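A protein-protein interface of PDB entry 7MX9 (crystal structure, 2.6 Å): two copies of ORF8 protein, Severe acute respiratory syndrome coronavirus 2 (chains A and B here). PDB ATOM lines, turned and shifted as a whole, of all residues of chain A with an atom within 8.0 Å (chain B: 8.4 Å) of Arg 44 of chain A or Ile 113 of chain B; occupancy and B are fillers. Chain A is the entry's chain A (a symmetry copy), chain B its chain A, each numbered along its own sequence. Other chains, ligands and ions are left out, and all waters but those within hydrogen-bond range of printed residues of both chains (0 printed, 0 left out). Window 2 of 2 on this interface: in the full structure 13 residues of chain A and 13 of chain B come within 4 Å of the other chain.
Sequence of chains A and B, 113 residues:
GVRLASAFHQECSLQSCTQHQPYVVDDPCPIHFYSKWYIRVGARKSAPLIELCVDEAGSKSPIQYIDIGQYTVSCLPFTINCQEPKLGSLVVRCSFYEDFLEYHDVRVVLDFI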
ATOM      1  N   ARG A  40     -11.759   9.501 -26.294  1.00  0.00           N
ATOM      2  CA  ARG A  40     -11.776   9.094 -24.899  1.00  0.00           C
ATOM      3  C   ARG A  40     -12.159   7.618 -24.809  1.00  0.00           C
ATOM      4  O   ARG A  40     -12.440   6.965 -25.813  1.00  0.00           O
ATOM      5  CB  ARG A  40     -12.716   9.986 -24.091  1.00  0.00           C
ATOM      6  CG  ARG A  40     -14.194   9.800 -24.353  1.00  0.00           C
ATOM      7  CD  ARG A  40     -14.959  11.051 -23.918  1.00  0.00           C
ATOM      8  NE  ARG A  40     -14.470  11.574 -22.640  1.00  0.00           N
ATOM      9  CZ  ARG A  40     -15.046  11.354 -21.461  1.00  0.00           C
ATOM     10  NH1 ARG A  40     -16.143  10.616 -21.383  1.00  0.00           N
ATOM     11  NH2 ARG A  40     -14.522  11.873 -20.358  1.00  0.00           N
ATOM     12  N   VAL A  41     -12.146   7.075 -23.595  1.00  0.00           N
ATOM     13  CA  VAL A  41     -12.424   5.662 -23.360  1.00  0.00           C
ATOM     14  C   VAL A  41     -13.590   5.565 -22.389  1.00  0.00           C
ATOM     15  O   VAL A  41     -13.498   6.035 -21.248  1.00  0.00           O
ATOM     16  CB  VAL A  41     -11.197   4.917 -22.814  1.00  0.00           C
ATOM     17  CG1 VAL A  41     -11.496   3.428 -22.680  1.00  0.00           C
ATOM     18  CG2 VAL A  41      -9.994   5.148 -23.718  1.00  0.00           C
ATOM     19  N   GLY A  42     -14.680   4.950 -22.835  1.00  0.00           N
ATOM     20  CA  GLY A  42     -15.854   4.816 -22.000  1.00  0.00           C
ATOM     21  C   GLY A  42     -16.590   6.127 -21.837  1.00  0.00           C
ATOM     22  O   GLY A  42     -16.117   7.175 -22.287  1.00  0.00           O
ATOM     23  N   ALA A  43     -17.758   6.079 -21.196  1.00  0.00           N
ATOM     24  CA  ALA A  43     -18.577   7.262 -20.964  1.00  0.00           C
ATOM     25  C   ALA A  43     -18.262   7.933 -19.636  1.00  0.00           C
ATOM     26  O   ALA A  43     -19.159   8.520 -19.016  1.00  0.00           O
ATOM     27  CB  ALA A  43     -20.060   6.891 -21.028  1.00  0.00           C
ATOM     28  N   ARG A  44     -17.013   7.875 -19.185  1.00  0.00           N
ATOM     29  CA  ARG A  44     -16.665   8.250 -17.824  1.00  0.00           C
ATOM     30  C   ARG A  44     -15.884   9.557 -17.808  1.00  0.00           C
ATOM     31  O   ARG A  44     -15.003   9.779 -18.644  1.00  0.00           O
ATOM     32  CB  ARG A  44     -15.872   7.133 -17.149  1.00  0.00           C
ATOM     33  CG  ARG A  44     -16.235   7.000 -15.694  1.00  0.00           C
ATOM     34  CD  ARG A  44     -16.002   5.611 -15.125  1.00  0.00           C
ATOM     35  NE  ARG A  44     -16.338   5.636 -13.705  1.00  0.00           N
ATOM     36  CZ  ARG A  44     -15.472   5.938 -12.745  1.00  0.00           C
ATOM     37  NH1 ARG A  44     -14.217   6.232 -13.054  1.00  0.00           N
ATOM     38  NH2 ARG A  44     -15.860   5.956 -11.477  1.00  0.00           N
ATOM     39  N   LYS A  45     -16.207  10.407 -16.828  1.00  0.00           N
ATOM     40  CA  LYS A  45     -15.765  11.798 -16.848  1.00  0.00           C
ATOM     41  C   LYS A  45     -14.260  11.905 -17.050  1.00  0.00           C
ATOM     42  O   LYS A  45     -13.790  12.581 -17.973  1.00  0.00           O
ATOM     43  CB  LYS A  45     -16.192  12.494 -15.553  1.00  0.00           C
ATOM     44  CG  LYS A  45     -16.260  14.012 -15.668  1.00  0.00           C
ATOM     45  CD  LYS A  45     -16.787  14.659 -14.393  1.00  0.00           C
ATOM     46  CE  LYS A  45     -16.899  16.170 -14.549  1.00  0.00           C
ATOM     47  NZ  LYS A  45     -15.599  16.792 -14.933  1.00  0.00           N
ATOM     48  N   SER A  46     -13.482  11.248 -16.190  1.00  0.00           N
ATOM     49  CA  SER A  46     -12.025  11.264 -16.302  1.00  0.00           C
ATOM     50  C   SER A  46     -11.573   9.949 -16.931  1.00  0.00           C
ATOM     51  O   SER A  46     -11.181   8.999 -16.254  1.00  0.00           O
ATOM     52  CB  SER A  46     -11.380  11.493 -14.938  1.00  0.00           C
ATOM     53  OG  SER A  46     -11.684  12.788 -14.447  1.00  0.00           O
ATOM     54  N   ALA A  47     -11.640   9.906 -18.260  1.00  0.00           N
ATOM     55  CA  ALA A  47     -11.189   8.764 -19.034  1.00  0.00           C
ATOM     56  C   ALA A  47      -9.899   9.105 -19.777  1.00  0.00           C
ATOM     57  O   ALA A  47      -9.668  10.268 -20.124  1.00  0.00           O
ATOM     58  CB  ALA A  47     -12.255   8.329 -20.047  1.00  0.00           C
ATOM     59  N   PRO A  48      -9.032   8.125 -20.022  1.00  0.00           N
ATOM     60  CA  PRO A  48      -7.819   8.403 -20.802  1.00  0.00           C
ATOM     61  C   PRO A  48      -8.165   8.809 -22.225  1.00  0.00           C
ATOM     62  O   PRO A  48      -9.207   8.435 -22.769  1.00  0.00           O
ATOM     63  CB  PRO A  48      -7.052   7.074 -20.765  1.00  0.00           C
ATOM     64  CG  PRO A  48      -8.090   6.029 -20.462  1.00  0.00           C
ATOM     65  CD  PRO A  48      -9.130   6.711 -19.614  1.00  0.00           C
ATOM     66  N   LEU A  49      -7.271   9.584 -22.832  1.00  0.00           N
ATOM     67  CA  LEU A  49      -7.500  10.159 -24.149  1.00  0.00           C
ATOM     68  C   LEU A  49      -6.441   9.680 -25.132  1.00  0.00           C
ATOM     69  O   LEU A  49      -5.250   9.630 -24.807  1.00  0.00           O
ATOM     70  CB  LEU A  49      -7.492  11.688 -24.085  1.00  0.00           C
ATOM     71  CG  LEU A  49      -8.501  12.325 -23.130  1.00  0.00           C
ATOM     72  CD1 LEU A  49      -8.047  13.717 -22.708  1.00  0.00           C
ATOM     73  CD2 LEU A  49      -9.879  12.379 -23.771  1.00  0.00           C
ATOM     74  N   ARG A 107     -17.138  17.625 -26.365  1.00  0.00           N
ATOM     75  CA  ARG A 107     -17.464  16.325 -26.928  1.00  0.00           C
ATOM     76  C   ARG A 107     -18.203  16.500 -28.247  1.00  0.00           C
ATOM     77  O   ARG A 107     -19.040  17.396 -28.393  1.00  0.00           O
ATOM     78  CB  ARG A 107     -18.317  15.499 -25.968  1.00  0.00           C
ATOM     79  CG  ARG A 107     -18.581  14.088 -26.494  1.00  0.00           C
ATOM     80  CD  ARG A 107     -19.039  13.120 -25.412  1.00  0.00           C
ATOM     81  NE  ARG A 107     -18.333  13.308 -24.147  1.00  0.00           N
ATOM     82  CZ  ARG A 107     -18.533  12.568 -23.062  1.00  0.00           C
ATOM     83  NH1 ARG A 107     -19.416  11.577 -23.085  1.00  0.00           N
ATOM     84  NH2 ARG A 107     -17.849  12.815 -21.954  1.00  0.00           N
ATOM     85  N   GLN B  15     -23.840  16.632 -19.449  1.00  0.00           N
ATOM     86  CA  GLN B  15     -24.132  16.678 -18.024  1.00  0.00           C
ATOM     87  C   GLN B  15     -23.399  15.549 -17.317  1.00  0.00           C
ATOM     88  O   GLN B  15     -23.290  14.439 -17.846  1.00  0.00           O
ATOM     89  CB  GLN B  15     -25.637  16.567 -17.766  1.00  0.00           C
ATOM     90  CG  GLN B  15     -26.488  17.495 -18.618  1.00  0.00           C
ATOM     91  CD  GLN B  15     -27.708  18.014 -17.882  1.00  0.00           C
ATOM     92  OE1 GLN B  15     -28.020  17.570 -16.777  1.00  0.00           O
ATOM     93  NE2 GLN B  15     -28.409  18.959 -18.498  1.00  0.00           N
ATOM     94  N   SER B  16     -22.906  15.834 -16.116  1.00  0.00           N
ATOM     95  CA  SER B  16     -22.135  14.881 -15.331  1.00  0.00           C
ATOM     96  C   SER B  16     -22.962  14.416 -14.142  1.00  0.00           C
ATOM     97  O   SER B  16     -23.572  15.235 -13.445  1.00  0.00           O
ATOM     98  CB  SER B  16     -20.821  15.505 -14.854  1.00  0.00           C
ATOM     99  OG  SER B  16     -20.079  16.021 -15.945  1.00  0.00           O
ATOM    100  N   CYS B  17     -22.981  13.104 -13.915  1.00  0.00           N
ATOM    101  CA  CYS B  17     -23.703  12.521 -12.796  1.00  0.00           C
ATOM    102  C   CYS B  17     -23.054  11.195 -12.430  1.00  0.00           C
ATOM    103  O   CYS B  17     -22.190  10.684 -13.146  1.00  0.00           O
ATOM    104  CB  CYS B  17     -25.190  12.330 -13.122  1.00  0.00           C
ATOM    105  SG  CYS B  17     -25.542  11.519 -14.699  1.00  0.00           S
ATOM    106  N   THR B  18     -23.482  10.641 -11.299  1.00  0.00           N
ATOM    107  CA  THR B  18     -22.962   9.371 -10.812  1.00  0.00           C
ATOM    108  C   THR B  18     -23.835   8.238 -11.335  1.00  0.00           C
ATOM    109  O   THR B  18     -25.042   8.205 -11.073  1.00  0.00           O
ATOM    110  CB  THR B  18     -22.915   9.354  -9.285  1.00  0.00           C
ATOM    111  OG1 THR B  18     -21.943  10.302  -8.826  1.00  0.00           O
ATOM    112  CG2 THR B  18     -22.551   7.966  -8.779  1.00  0.00           C
ATOM    113  N   GLN B  19     -23.218   7.305 -12.055  1.00  0.00           N
ATOM    114  CA  GLN B  19     -23.969   6.274 -12.757  1.00  0.00           C
ATOM    115  C   GLN B  19     -24.858   5.485 -11.805  1.00  0.00           C
ATOM    116  O   GLN B  19     -24.492   5.217 -10.658  1.00  0.00           O
ATOM    117  CB  GLN B  19     -23.005   5.329 -13.474  1.00  0.00           C
ATOM    118  CG  GLN B  19     -23.680   4.205 -14.232  1.00  0.00           C
ATOM    119  CD  GLN B  19     -22.880   3.766 -15.440  1.00  0.00           C
ATOM    120  OE1 GLN B  19     -23.300   3.961 -16.580  1.00  0.00           O
ATOM    121  NE2 GLN B  19     -21.718   3.172 -15.197  1.00  0.00           N
ATOM    122  N   TYR B  23     -30.601  11.462 -10.430  1.00  0.00           N
ATOM    123  CA  TYR B  23     -29.984  12.695 -10.904  1.00  0.00           C
ATOM    124  C   TYR B  23     -31.067  13.616 -11.439  1.00  0.00           C
ATOM    125  O   TYR B  23     -31.820  13.231 -12.339  1.00  0.00           O
ATOM    126  CB  TYR B  23     -28.949  12.408 -11.990  1.00  0.00           C
ATOM    127  CG  TYR B  23     -28.401  13.653 -12.645  1.00  0.00           C
ATOM    128  CD1 TYR B  23     -27.805  14.651 -11.889  1.00  0.00           C
ATOM    129  CD2 TYR B  23     -28.488  13.835 -14.018  1.00  0.00           C
ATOM    130  CE1 TYR B  23     -27.302  15.792 -12.481  1.00  0.00           C
ATOM    131  CE2 TYR B  23     -27.989  14.975 -14.622  1.00  0.00           C
ATOM    132  CZ  TYR B  23     -27.398  15.949 -13.847  1.00  0.00           C
ATOM    133  OH  TYR B  23     -26.901  17.086 -14.438  1.00  0.00           O
ATOM    134  N   CYS B  82     -29.046   7.988 -13.396  1.00  0.00           N
ATOM    135  CA  CYS B  82     -27.951   8.442 -14.261  1.00  0.00           C
ATOM    136  C   CYS B  82     -27.389   7.275 -15.069  1.00  0.00           C
ATOM    137  O   CYS B  82     -26.388   6.649 -14.703  1.00  0.00           O
ATOM    138  CB  CYS B  82     -26.867   9.129 -13.417  1.00  0.00           C
ATOM    139  SG  CYS B  82     -25.370   9.537 -14.315  1.00  0.00           S
ATOM    140  N   LEU B 110     -24.609  12.139 -21.170  1.00  0.00           N
ATOM    141  CA  LEU B 110     -24.067  12.037 -19.827  1.00  0.00           C
ATOM    142  C   LEU B 110     -22.658  11.454 -19.851  1.00  0.00           C
ATOM    143  O   LEU B 110     -22.314  10.651 -20.724  1.00  0.00           O
ATOM    144  CB  LEU B 110     -24.952  11.144 -18.952  1.00  0.00           C
ATOM    145  CG  LEU B 110     -26.467  11.340 -18.919  1.00  0.00           C
ATOM    146  CD1 LEU B 110     -27.125  10.159 -18.210  1.00  0.00           C
ATOM    147  CD2 LEU B 110     -26.807  12.638 -18.223  1.00  0.00           C
ATOM    148  N   ASP B 111     -21.849  11.866 -18.878  1.00  0.00           N
ATOM    149  CA  ASP B 111     -20.608  11.184 -18.532  1.00  0.00           C
ATOM    150  C   ASP B 111     -20.574  11.017 -17.019  1.00  0.00           C
ATOM    151  O   ASP B 111     -21.221  11.763 -16.280  1.00  0.00           O
ATOM    152  CB  ASP B 111     -19.362  11.928 -19.039  1.00  0.00           C
ATOM    153  CG  ASP B 111     -19.269  13.345 -18.532  1.00  0.00           C
ATOM    154  OD1 ASP B 111     -19.901  13.669 -17.506  1.00  0.00           O
ATOM    155  OD2 ASP B 111     -18.555  14.138 -19.176  1.00  0.00           O
ATOM    156  N   PHE B 112     -19.823  10.024 -16.559  1.00  0.00           N
ATOM    157  CA  PHE B 112     -19.996   9.491 -15.213  1.00  0.00           C
ATOM    158  C   PHE B 112     -18.810   9.833 -14.321  1.00  0.00           C
ATOM    159  O   PHE B 112     -17.708   9.309 -14.505  1.00  0.00           O
ATOM    160  CB  PHE B 112     -20.207   7.978 -15.275  1.00  0.00           C
ATOM    161  CG  PHE B 112     -21.343   7.564 -16.165  1.00  0.00           C
ATOM    162  CD1 PHE B 112     -22.639   7.945 -15.870  1.00  0.00           C
ATOM    163  CD2 PHE B 112     -21.119   6.797 -17.299  1.00  0.00           C
ATOM    164  CE1 PHE B 112     -23.690   7.571 -16.680  1.00  0.00           C
ATOM    165  CE2 PHE B 112     -22.171   6.420 -18.116  1.00  0.00           C
ATOM    166  CZ  PHE B 112     -23.456   6.808 -17.805  1.00  0.00           C
ATOM    167  N   ILE B 113     -19.051  10.712 -13.352  1.00  0.00           N
ATOM    168  CA  ILE B 113     -18.195  10.873 -12.187  1.00  0.00           C
ATOM    169  C   ILE B 113     -18.650   9.881 -11.127  1.00  0.00           C
ATOM    170  O   ILE B 113     -18.286   8.704 -11.146  1.00  0.00           O
ATOM    171  CB  ILE B 113     -18.238  12.314 -11.650  1.00  0.00           C
ATOM    172  CG1 ILE B 113     -17.355  12.436 -10.402  1.00  0.00           C
ATOM    173  CG2 ILE B 113     -19.663  12.744 -11.365  1.00  0.00           C
ATOM    174  CD1 ILE B 113     -15.884  12.177 -10.626  1.00  0.00           C
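No position is printed for both chains. Of the 9 pairs that touch across the chains among the printed residues, none has its exchanged pair printed and touching as well.
The backbone NH (N) of Phe 112 of chain B sits at hydrogen-bond distance from the backbone carbonyl oxygen (O) of Ala 43 of chain A, 3.0 Å away. The backbone carbonyl oxygen (O) of Phe 112 of chain B sits at hydrogen-bond distance from the backbone NH (N) of Lys 45 of chain A, at 3.0 Å. The side-chain carboxylate of Asp 111 of chain B lies within salt-bridge range of the guanidinium group of Arg 107 of chain A, at 3.2 Å.
Of chain B, only Phe 112 (3.0 Å) and Ile 113 (3.7 Å) come within 4 Å of Arg 44 of chain A. Of chain A, only Arg 44 (3.7 Å) and Lys 45 (3.9 Å) come within 4 Å of Ile 113 of chain B. Of the printed residues of chain B, Arg 107 of chain A touches Leu 110 (3.9 Å) and Asp 111 (3.2 Å). Printed residues of chain B within 4 Å of Lys 45 of chain A: Ser 16, Phe 112 and Ile 113. Gly 42 of chain A touches none of the printed residues of chain B. The nearest residue of chain B that does not touch Arg 44 of chain A is Asp 111 of chain B (4.4 Å). The nearest residue of chain A that does not touch Ile 113 of chain B is Ser 46 of chain A (5.7 Å).
The backbone NH (N) of Ile 113 of chain B is in hydrogen-bond range of the backbone carbonyl oxygen (O) of Cys 17 of chain B (3.1 Å). OD1 of Asp 111 of chain B is in hydrogen-bond range of OG of Ser 16 of chain B. The backbone carbonyl oxygen of Asp 111 of chain B is in hydrogen-bond range of the backbone NH of Cys 17 of chain B (3.2 Å). The side-chain sulfur (SG) of Cys 17 of chain B is disulfide-bonded to the side-chain sulfur (SG) of Cys 82 of chain B, at 2.0 Å. The backbone carbonyl oxygen of Gln 15 of chain B is in hydrogen-bond range of the backbone NH of Asp 111 of chain B (3.1 Å). The guanidinium group (NH2) of Arg 40 of chain A lies within hydrogen-bond range of the backbone carbonyl oxygen (O) of Arg 44 of chain A (2.7 Å).
Of the 11 printed residues of chain A, 4 touch a printed residue of chain B. Hydrophobic or aromatic side chains of chain A within 4 Å of the printed part of chain B: Ala 43. Hydrophobic or aromatic side chains of chain B within 4 Å of the printed part of chain A: Phe 112 and Ile 113. Among the printed residues, Asp or Glu carboxylates within 4 Å of a Lys or Arg side-chain nitrogen of the other chain: Arg 107 of chain A with Asp 111 of chain B.
Among the printed residues, merely in contact across the chains: Ala 43 of chain A with Asp 111 of chain B, Arg 44 of chain A with Phe 112 of chain B, Arg 44 of chain A with Ile 113 of chain B, Lys 45 of chain A with Ser 16 of chain B, Lys 45 of chain A with Ile 113 of chain B and Arg 107 of chain A with Leu 110 of chain B.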
